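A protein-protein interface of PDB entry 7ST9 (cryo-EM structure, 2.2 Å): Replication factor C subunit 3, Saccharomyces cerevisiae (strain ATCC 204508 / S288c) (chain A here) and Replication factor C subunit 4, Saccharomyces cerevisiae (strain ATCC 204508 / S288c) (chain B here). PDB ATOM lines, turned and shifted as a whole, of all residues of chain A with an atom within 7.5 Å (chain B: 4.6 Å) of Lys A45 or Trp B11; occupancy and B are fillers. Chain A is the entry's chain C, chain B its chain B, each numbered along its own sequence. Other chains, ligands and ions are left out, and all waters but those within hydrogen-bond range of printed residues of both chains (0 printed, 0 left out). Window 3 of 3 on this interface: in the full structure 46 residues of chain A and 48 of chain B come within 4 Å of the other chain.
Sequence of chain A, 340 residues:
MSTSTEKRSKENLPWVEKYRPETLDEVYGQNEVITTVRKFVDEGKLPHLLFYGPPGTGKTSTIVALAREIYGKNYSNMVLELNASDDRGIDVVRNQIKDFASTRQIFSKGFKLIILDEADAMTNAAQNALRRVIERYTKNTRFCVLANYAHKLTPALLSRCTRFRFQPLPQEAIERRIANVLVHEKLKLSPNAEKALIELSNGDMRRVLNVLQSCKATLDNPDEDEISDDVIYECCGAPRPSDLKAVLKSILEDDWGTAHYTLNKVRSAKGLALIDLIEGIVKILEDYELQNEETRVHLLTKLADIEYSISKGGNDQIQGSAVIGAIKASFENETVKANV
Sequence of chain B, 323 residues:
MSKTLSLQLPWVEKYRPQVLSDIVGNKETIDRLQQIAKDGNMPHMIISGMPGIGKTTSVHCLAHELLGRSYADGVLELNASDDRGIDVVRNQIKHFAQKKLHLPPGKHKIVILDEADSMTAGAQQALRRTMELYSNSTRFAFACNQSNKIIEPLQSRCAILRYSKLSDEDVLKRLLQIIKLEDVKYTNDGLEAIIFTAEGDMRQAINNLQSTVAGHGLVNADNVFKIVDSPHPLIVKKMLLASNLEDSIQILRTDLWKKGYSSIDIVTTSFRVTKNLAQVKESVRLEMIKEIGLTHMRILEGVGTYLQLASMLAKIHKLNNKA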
ATOM      1  N   LYS A  39      -0.867  27.953  29.811  1.00  0.00           N
ATOM      2  CA  LYS A  39       0.157  28.893  29.380  1.00  0.00           C
ATOM      3  C   LYS A  39       0.670  28.563  27.983  1.00  0.00           C
ATOM      4  O   LYS A  39       1.041  29.471  27.229  1.00  0.00           O
ATOM      5  CB  LYS A  39       1.281  28.894  30.404  1.00  0.00           C
ATOM      6  CG  LYS A  39       2.514  29.688  30.027  1.00  0.00           C
ATOM      7  CD  LYS A  39       3.527  29.680  31.163  1.00  0.00           C
ATOM      8  CE  LYS A  39       3.693  28.282  31.746  1.00  0.00           C
ATOM      9  NZ  LYS A  39       3.904  27.278  30.652  1.00  0.00           N
ATOM     10  N   PHE A  40       0.685  27.280  27.611  1.00  0.00           N
ATOM     11  CA  PHE A  40       1.050  26.911  26.248  1.00  0.00           C
ATOM     12  C   PHE A  40       0.078  27.514  25.242  1.00  0.00           C
ATOM     13  O   PHE A  40       0.491  28.075  24.220  1.00  0.00           O
ATOM     14  CB  PHE A  40       1.086  25.387  26.106  1.00  0.00           C
ATOM     15  CG  PHE A  40       2.458  24.793  26.252  1.00  0.00           C
ATOM     16  CD1 PHE A  40       3.462  25.099  25.348  1.00  0.00           C
ATOM     17  CD2 PHE A  40       2.741  23.918  27.288  1.00  0.00           C
ATOM     18  CE1 PHE A  40       4.723  24.550  25.480  1.00  0.00           C
ATOM     19  CE2 PHE A  40       3.999  23.366  27.424  1.00  0.00           C
ATOM     20  CZ  PHE A  40       4.992  23.681  26.520  1.00  0.00           C
ATOM     21  N   VAL A  41      -1.225  27.406  25.513  1.00  0.00           N
ATOM     22  CA  VAL A  41      -2.205  27.986  24.597  1.00  0.00           C
ATOM     23  C   VAL A  41      -2.120  29.508  24.633  1.00  0.00           C
ATOM     24  O   VAL A  41      -2.307  30.178  23.610  1.00  0.00           O
ATOM     25  CB  VAL A  41      -3.633  27.493  24.909  1.00  0.00           C
ATOM     26  CG1 VAL A  41      -3.990  27.691  26.368  1.00  0.00           C
ATOM     27  CG2 VAL A  41      -4.646  28.198  24.015  1.00  0.00           C
ATOM     28  N   ASP A  42      -1.834  30.077  25.807  1.00  0.00           N
ATOM     29  CA  ASP A  42      -1.656  31.524  25.897  1.00  0.00           C
ATOM     30  C   ASP A  42      -0.522  31.990  24.995  1.00  0.00           C
ATOM     31  O   ASP A  42      -0.634  33.029  24.332  1.00  0.00           O
ATOM     32  CB  ASP A  42      -1.387  31.927  27.346  1.00  0.00           C
ATOM     33  CG  ASP A  42      -1.177  33.420  27.506  1.00  0.00           C
ATOM     34  OD1 ASP A  42      -1.868  34.197  26.814  1.00  0.00           O
ATOM     35  OD2 ASP A  42      -0.321  33.817  28.324  1.00  0.00           O
ATOM     36  N   GLU A  43       0.577  31.241  24.957  1.00  0.00           N
ATOM     37  CA  GLU A  43       1.695  31.555  24.078  1.00  0.00           C
ATOM     38  C   GLU A  43       1.555  30.929  22.696  1.00  0.00           C
ATOM     39  O   GLU A  43       2.405  31.175  21.833  1.00  0.00           O
ATOM     40  CB  GLU A  43       3.011  31.095  24.713  1.00  0.00           C
ATOM     41  CG  GLU A  43       4.225  31.905  24.283  1.00  0.00           C
ATOM     42  CD  GLU A  43       5.141  32.245  25.442  1.00  0.00           C
ATOM     43  OE1 GLU A  43       6.047  31.439  25.742  1.00  0.00           O
ATOM     44  OE2 GLU A  43       4.955  33.318  26.054  1.00  0.00           O
ATOM     45  N   GLY A  44       0.516  30.133  22.464  1.00  0.00           N
ATOM     46  CA  GLY A  44       0.312  29.536  21.152  1.00  0.00           C
ATOM     47  C   GLY A  44       1.459  28.660  20.698  1.00  0.00           C
ATOM     48  O   GLY A  44       1.874  28.737  19.536  1.00  0.00           O
ATOM     49  N   LYS A  45       1.983  27.825  21.593  1.00  0.00           N
ATOM     50  CA  LYS A  45       3.121  26.954  21.309  1.00  0.00           C
ATOM     51  C   LYS A  45       2.824  25.532  21.765  1.00  0.00           C
ATOM     52  O   LYS A  45       3.640  24.870  22.411  1.00  0.00           O
ATOM     53  CB  LYS A  45       4.382  27.491  21.979  1.00  0.00           C
ATOM     54  CG  LYS A  45       5.026  28.649  21.238  1.00  0.00           C
ATOM     55  CD  LYS A  45       6.126  29.300  22.060  1.00  0.00           C
ATOM     56  CE  LYS A  45       7.333  28.389  22.201  1.00  0.00           C
ATOM     57  NZ  LYS A  45       8.458  29.057  22.911  1.00  0.00           N
ATOM     58  N   LEU A  46       1.641  25.040  21.423  1.00  0.00           N
ATOM     59  CA  LEU A  46       1.231  23.714  21.867  1.00  0.00           C
ATOM     60  C   LEU A  46       2.057  22.642  21.163  1.00  0.00           C
ATOM     61  O   LEU A  46       2.108  22.620  19.928  1.00  0.00           O
ATOM     62  CB  LEU A  46      -0.254  23.498  21.585  1.00  0.00           C
ATOM     63  CG  LEU A  46      -0.929  22.397  22.406  1.00  0.00           C
ATOM     64  CD1 LEU A  46      -1.140  22.851  23.842  1.00  0.00           C
ATOM     65  CD2 LEU A  46      -2.248  21.987  21.768  1.00  0.00           C
ATOM     66  N   PRO A  47       2.725  21.746  21.901  1.00  0.00           N
ATOM     67  CA  PRO A  47       3.389  20.610  21.252  1.00  0.00           C
ATOM     68  C   PRO A  47       2.476  19.398  21.156  1.00  0.00           C
ATOM     69  O   PRO A  47       1.334  19.444  21.623  1.00  0.00           O
ATOM     70  CB  PRO A  47       4.586  20.344  22.169  1.00  0.00           C
ATOM     71  CG  PRO A  47       4.086  20.723  23.530  1.00  0.00           C
ATOM     72  CD  PRO A  47       3.027  21.796  23.344  1.00  0.00           C
ATOM     73  N   HIS A  48       2.960  18.315  20.553  1.00  0.00           N
ATOM     74  CA  HIS A  48       2.217  17.063  20.583  1.00  0.00           C
ATOM     75  C   HIS A  48       2.132  16.558  22.017  1.00  0.00           C
ATOM     76  O   HIS A  48       3.134  16.531  22.738  1.00  0.00           O
ATOM     77  CB  HIS A  48       2.890  16.024  19.685  1.00  0.00           C
ATOM     78  CG  HIS A  48       3.158  16.512  18.296  1.00  0.00           C
ATOM     79  ND1 HIS A  48       2.155  16.724  17.375  1.00  0.00           N
ATOM     80  CD2 HIS A  48       4.315  16.836  17.671  1.00  0.00           C
ATOM     81  CE1 HIS A  48       2.682  17.156  16.243  1.00  0.00           C
ATOM     82  NE2 HIS A  48       3.991  17.232  16.396  1.00  0.00           N
ATOM     83  N   LEU A  49       0.933  16.158  22.432  1.00  0.00           N
ATOM     84  CA  LEU A  49       0.653  15.864  23.829  1.00  0.00           C
ATOM     85  C   LEU A  49       0.311  14.394  24.023  1.00  0.00           C
ATOM     86  O   LEU A  49      -0.296  13.756  23.158  1.00  0.00           O
ATOM     87  CB  LEU A  49      -0.510  16.720  24.352  1.00  0.00           C
ATOM     88  CG  LEU A  49      -0.315  18.236  24.325  1.00  0.00           C
ATOM     89  CD1 LEU A  49      -1.641  18.942  24.554  1.00  0.00           C
ATOM     90  CD2 LEU A  49       0.708  18.670  25.363  1.00  0.00           C
ATOM     91  N   PHE A 111      -3.443  26.361  13.991  1.00  0.00           N
ATOM     92  CA  PHE A 111      -3.213  24.965  13.652  1.00  0.00           C
ATOM     93  C   PHE A 111      -4.438  24.120  13.978  1.00  0.00           C
ATOM     94  O   PHE A 111      -5.294  24.499  14.780  1.00  0.00           O
ATOM     95  CB  PHE A 111      -1.989  24.419  14.397  1.00  0.00           C
ATOM     96  CG  PHE A 111      -2.042  24.618  15.887  1.00  0.00           C
ATOM     97  CD1 PHE A 111      -2.859  23.827  16.678  1.00  0.00           C
ATOM     98  CD2 PHE A 111      -1.271  25.593  16.496  1.00  0.00           C
ATOM     99  CE1 PHE A 111      -2.909  24.008  18.046  1.00  0.00           C
ATOM    100  CE2 PHE A 111      -1.316  25.779  17.864  1.00  0.00           C
ATOM    101  CZ  PHE A 111      -2.136  24.985  18.640  1.00  0.00           C
ATOM    102  N   ARG A 142      -1.410  19.473  15.330  1.00  0.00           N
ATOM    103  CA  ARG A 142      -0.868  18.950  16.576  1.00  0.00           C
ATOM    104  C   ARG A 142      -1.705  17.760  17.019  1.00  0.00           C
ATOM    105  O   ARG A 142      -2.935  17.783  16.918  1.00  0.00           O
ATOM    106  CB  ARG A 142      -0.848  20.019  17.679  1.00  0.00           C
ATOM    107  CG  ARG A 142      -0.110  21.297  17.309  1.00  0.00           C
ATOM    108  CD  ARG A 142       1.387  21.067  17.136  1.00  0.00           C
ATOM    109  NE  ARG A 142       1.963  21.955  16.133  1.00  0.00           N
ATOM    110  CZ  ARG A 142       2.182  23.251  16.314  1.00  0.00           C
ATOM    111  NH1 ARG A 142       1.895  23.848  17.459  1.00  0.00           N
ATOM    112  NH2 ARG A 142       2.706  23.964  15.322  1.00  0.00           N
ATOM    113  N   GLN B   8       4.561  29.463  16.392  1.00  0.00           N
ATOM    114  CA  GLN B   8       5.945  29.052  16.593  1.00  0.00           C
ATOM    115  C   GLN B   8       6.021  27.534  16.687  1.00  0.00           C
ATOM    116  O   GLN B   8       5.296  26.917  17.473  1.00  0.00           O
ATOM    117  CB  GLN B   8       6.526  29.690  17.854  1.00  0.00           C
ATOM    118  CG  GLN B   8       6.655  31.202  17.776  1.00  0.00           C
ATOM    119  CD  GLN B   8       7.734  31.641  16.805  1.00  0.00           C
ATOM    120  OE1 GLN B   8       8.764  30.982  16.664  1.00  0.00           O
ATOM    121  NE2 GLN B   8       7.502  32.761  16.128  1.00  0.00           N
ATOM    122  N   LEU B   9       6.906  26.943  15.891  1.00  0.00           N
ATOM    123  CA  LEU B   9       7.045  25.500  15.865  1.00  0.00           C
ATOM    124  C   LEU B   9       7.579  25.001  17.209  1.00  0.00           C
ATOM    125  O   LEU B   9       8.289  25.727  17.910  1.00  0.00           O
ATOM    126  CB  LEU B   9       8.002  25.084  14.749  1.00  0.00           C
ATOM    127  CG  LEU B   9       7.470  24.736  13.351  1.00  0.00           C
ATOM    128  CD1 LEU B   9       8.432  23.783  12.655  1.00  0.00           C
ATOM    129  CD2 LEU B   9       6.070  24.145  13.358  1.00  0.00           C
ATOM    130  N   PRO B  10       7.246  23.770  17.598  1.00  0.00           N
ATOM    131  CA  PRO B  10       7.893  23.185  18.776  1.00  0.00           C
ATOM    132  C   PRO B  10       9.385  23.010  18.542  1.00  0.00           C
ATOM    133  O   PRO B  10       9.842  22.818  17.414  1.00  0.00           O
ATOM    134  CB  PRO B  10       7.182  21.837  18.948  1.00  0.00           C
ATOM    135  CG  PRO B  10       6.566  21.545  17.628  1.00  0.00           C
ATOM    136  CD  PRO B  10       6.236  22.868  17.018  1.00  0.00           C
ATOM    137  N   TRP B  11      10.149  23.081  19.635  1.00  0.00           N
ATOM    138  CA  TRP B  11      11.604  23.090  19.521  1.00  0.00           C
ATOM    139  C   TRP B  11      12.135  21.817  18.872  1.00  0.00           C
ATOM    140  O   TRP B  11      13.187  21.849  18.223  1.00  0.00           O
ATOM    141  CB  TRP B  11      12.231  23.283  20.901  1.00  0.00           C
ATOM    142  CG  TRP B  11      12.066  24.671  21.453  1.00  0.00           C
ATOM    143  CD1 TRP B  11      11.501  25.744  20.827  1.00  0.00           C
ATOM    144  CD2 TRP B  11      12.479  25.133  22.744  1.00  0.00           C
ATOM    145  NE1 TRP B  11      11.534  26.844  21.649  1.00  0.00           N
ATOM    146  CE2 TRP B  11      12.130  26.495  22.832  1.00  0.00           C
ATOM    147  CE3 TRP B  11      13.109  24.527  23.835  1.00  0.00           C
ATOM    148  CZ2 TRP B  11      12.388  27.260  23.967  1.00  0.00           C
ATOM    149  CZ3 TRP B  11      13.366  25.288  24.960  1.00  0.00           C
ATOM    150  CH2 TRP B  11      13.006  26.640  25.017  1.00  0.00           C
ATOM    151  N   VAL B  12      11.433  20.692  19.030  1.00  0.00           N
ATOM    152  CA  VAL B  12      11.909  19.444  18.434  1.00  0.00           C
ATOM    153  C   VAL B  12      11.997  19.579  16.919  1.00  0.00           C
ATOM    154  O   VAL B  12      12.978  19.151  16.299  1.00  0.00           O
ATOM    155  CB  VAL B  12      11.005  18.261  18.840  1.00  0.00           C
ATOM    156  CG1 VAL B  12      11.393  17.746  20.217  1.00  0.00           C
ATOM    157  CG2 VAL B  12       9.528  18.644  18.790  1.00  0.00           C
ATOM    158  N   GLU B  13      10.978  20.172  16.300  1.00  0.00           N
ATOM    159  CA  GLU B  13      10.972  20.367  14.856  1.00  0.00           C
ATOM    160  C   GLU B  13      11.656  21.659  14.437  1.00  0.00           C
ATOM    161  O   GLU B  13      12.233  21.719  13.345  1.00  0.00           O
ATOM    162  CB  GLU B  13       9.531  20.360  14.334  1.00  0.00           C
ATOM    163  CG  GLU B  13       9.398  20.189  12.825  1.00  0.00           C
ATOM    164  CD  GLU B  13      10.199  19.018  12.287  1.00  0.00           C
ATOM    165  OE1 GLU B  13       9.684  17.880  12.313  1.00  0.00           O
ATOM    166  OE2 GLU B  13      11.344  19.236  11.838  1.00  0.00           O
ATOM    167  N   LYS B  14      11.604  22.693  15.278  1.00  0.00           N
ATOM    168  CA  LYS B  14      12.237  23.960  14.930  1.00  0.00           C
ATOM    169  C   LYS B  14      13.747  23.807  14.797  1.00  0.00           C
ATOM    170  O   LYS B  14      14.357  24.377  13.885  1.00  0.00           O
ATOM    171  CB  LYS B  14      11.897  25.018  15.979  1.00  0.00           C
ATOM    172  CG  LYS B  14      12.509  26.382  15.705  1.00  0.00           C
ATOM    173  CD  LYS B  14      12.029  27.418  16.708  1.00  0.00           C
ATOM    174  CE  LYS B  14      12.582  28.796  16.391  1.00  0.00           C
ATOM    175  NZ  LYS B  14      12.073  29.833  17.330  1.00  0.00           N
ATOM    176  N   TYR B  15      14.365  23.043  15.697  1.00  0.00           N
ATOM    177  CA  TYR B  15      15.815  22.913  15.757  1.00  0.00           C
ATOM    178  C   TYR B  15      16.300  21.568  15.220  1.00  0.00           C
ATOM    179  O   TYR B  15      17.347  21.068  15.637  1.00  0.00           O
ATOM    180  CB  TYR B  15      16.302  23.127  17.190  1.00  0.00           C
ATOM    181  CG  TYR B  15      16.207  24.567  17.637  1.00  0.00           C
ATOM    182  CD1 TYR B  15      16.963  25.555  17.019  1.00  0.00           C
ATOM    183  CD2 TYR B  15      15.354  24.944  18.665  1.00  0.00           C
ATOM    184  CE1 TYR B  15      16.878  26.873  17.417  1.00  0.00           C
ATOM    185  CE2 TYR B  15      15.264  26.262  19.070  1.00  0.00           C
ATOM    186  CZ  TYR B  15      16.028  27.222  18.441  1.00  0.00           C
ATOM    187  OH  TYR B  15      15.945  28.536  18.836  1.00  0.00           O
ATOM    188  N   ILE B 178      20.960  24.793  21.982  1.00  0.00           N
ATOM    189  CA  ILE B 178      19.565  25.210  21.858  1.00  0.00           C
ATOM    190  C   ILE B 178      19.256  26.335  22.837  1.00  0.00           C
ATOM    191  O   ILE B 178      18.541  27.286  22.505  1.00  0.00           O
ATOM    192  CB  ILE B 178      18.621  24.010  22.063  1.00  0.00           C
ATOM    193  CG1 ILE B 178      18.834  22.942  20.982  1.00  0.00           C
ATOM    194  CG2 ILE B 178      17.168  24.470  22.064  1.00  0.00           C
ATOM    195  CD1 ILE B 178      18.952  23.480  19.574  1.00  0.00           C
ATOM    196  N   GLU B 182      17.920  30.059  22.034  1.00  0.00           N
ATOM    197  CA  GLU B 182      16.653  30.518  22.590  1.00  0.00           C
ATOM    198  C   GLU B 182      16.815  31.500  23.743  1.00  0.00           C
ATOM    199  O   GLU B 182      15.818  32.088  24.174  1.00  0.00           O
ATOM    200  CB  GLU B 182      15.825  29.321  23.075  1.00  0.00           C
ATOM    201  CG  GLU B 182      15.126  28.553  21.967  1.00  0.00           C
ATOM    202  CD  GLU B 182      13.959  29.316  21.369  1.00  0.00           C
ATOM    203  OE1 GLU B 182      13.560  30.350  21.945  1.00  0.00           O
ATOM    204  OE2 GLU B 182      13.441  28.882  20.318  1.00  0.00           O
ATOM    205  N   VAL B 184      17.673  30.930  27.043  1.00  0.00           N
ATOM    206  CA  VAL B 184      16.913  30.315  28.125  1.00  0.00           C
ATOM    207  C   VAL B 184      17.749  30.350  29.396  1.00  0.00           C
ATOM    208  O   VAL B 184      18.913  29.931  29.396  1.00  0.00           O
ATOM    209  CB  VAL B 184      16.513  28.872  27.769  1.00  0.00           C
ATOM    210  CG1 VAL B 184      16.227  28.059  29.027  1.00  0.00           C
ATOM    211  CG2 VAL B 184      15.306  28.869  26.843  1.00  0.00           C
ATOM    212  N   ILE B 206      14.510  17.378  24.276  1.00  0.00           N
ATOM    213  CA  ILE B 206      14.107  18.687  23.776  1.00  0.00           C
ATOM    214  C   ILE B 206      12.662  18.984  24.159  1.00  0.00           C
ATOM    215  O   ILE B 206      12.324  20.116  24.526  1.00  0.00           O
ATOM    216  CB  ILE B 206      14.321  18.767  22.253  1.00  0.00           C
ATOM    217  CG1 ILE B 206      15.815  18.720  21.927  1.00  0.00           C
ATOM    218  CG2 ILE B 206      13.704  20.041  21.693  1.00  0.00           C
ATOM    219  CD1 ILE B 206      16.117  18.313  20.504  1.00  0.00           C
ATOM    220  N   LEU B 209      12.694  19.929  27.792  1.00  0.00           N
ATOM    221  CA  LEU B 209      13.285  21.252  27.962  1.00  0.00           C
ATOM    222  C   LEU B 209      12.294  22.344  27.587  1.00  0.00           C
ATOM    223  O   LEU B 209      12.155  23.339  28.306  1.00  0.00           O
ATOM    224  CB  LEU B 209      14.559  21.372  27.124  1.00  0.00           C
ATOM    225  CG  LEU B 209      15.303  22.708  27.212  1.00  0.00           C
ATOM    226  CD1 LEU B 209      16.134  22.781  28.483  1.00  0.00           C
ATOM    227  CD2 LEU B 209      16.179  22.915  25.987  1.00  0.00           C
ATOM    228  N   GLN B 210      11.595  22.177  26.461  1.00  0.00           N
ATOM    229  CA  GLN B 210      10.601  23.169  26.063  1.00  0.00           C
ATOM    230  C   GLN B 210       9.473  23.255  27.083  1.00  0.00           C
ATOM    231  O   GLN B 210       9.030  24.353  27.442  1.00  0.00           O
ATOM    232  CB  GLN B 210      10.044  22.828  24.681  1.00  0.00           C
ATOM    233  CG  GLN B 210       8.898  23.726  24.237  1.00  0.00           C
ATOM    234  CD  GLN B 210       8.486  23.475  22.803  1.00  0.00           C
ATOM    235  OE1 GLN B 210       9.166  23.894  21.867  1.00  0.00           O
ATOM    236  NE2 GLN B 210       7.367  22.783  22.621  1.00  0.00           N
ATOM    237  N   VAL B 213      10.799  25.100  30.146  1.00  0.00           N
ATOM    238  CA  VAL B 213      11.005  26.519  29.877  1.00  0.00           C
ATOM    239  C   VAL B 213       9.672  27.249  29.862  1.00  0.00           C
ATOM    240  O   VAL B 213       9.536  28.337  30.435  1.00  0.00           O
ATOM    241  CB  VAL B 213      11.768  26.706  28.553  1.00  0.00           C
ATOM    242  CG1 VAL B 213      11.636  28.140  28.055  1.00  0.00           C
ATOM    243  CG2 VAL B 213      13.228  26.329  28.729  1.00  0.00           C
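The side-chain carboxylate (OE2) of Glu B182 lies within hydrogen-bond range of the indole nitrogen (NE1) of Trp B11 (3.1 Å). The backbone NH (N) of Trp B11 is in hydrogen-bond range of the side-chain amide oxygen (OE1) of Gln B210, at 2.6 Å. O of Phe A40 is in hydrogen-bond range of N of Lys A45 (3.0 Å). The backbone carbonyl oxygen of Leu A46 sits at hydrogen-bond distance from the guanidinium group of Arg A142.
Among the printed residues, merely in contact across the chains: Lys A45 with Gln B8 (3.8 Å), Lys A45 with Trp B11 (3.99 Å), Pro A47 with Gln B210 (3.7 Å) and Arg A142 with Leu B9 (3.9 Å).
Of the printed residues of chain B, Lys A45 touches Gln B8 and Trp B11. Of the printed residues of chain A, Gln B8 touches Lys A45. Printed residues of chain A within 4 Å of Leu B9: Arg A142 (3.9 Å). Of the printed residues of chain B, Pro A47 touches Gln B210. Printed residues of chain B within 4 Å of Arg A142: Leu B9 (3.9 Å). The nearest printed residue of chain A that does not touch Trp B11 is Pro A47 (6.7 Å). The nearest printed residue of chain A that does not touch Gln B210 is Phe A40 (4.2 Å).
Hydrophobic or aromatic side chains of chain A within 4 Å of the printed part of chain B: Pro A47. Hydrophobic or aromatic side chains of chain B that line the printed part of chain A: Leu B9 and Trp B11.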
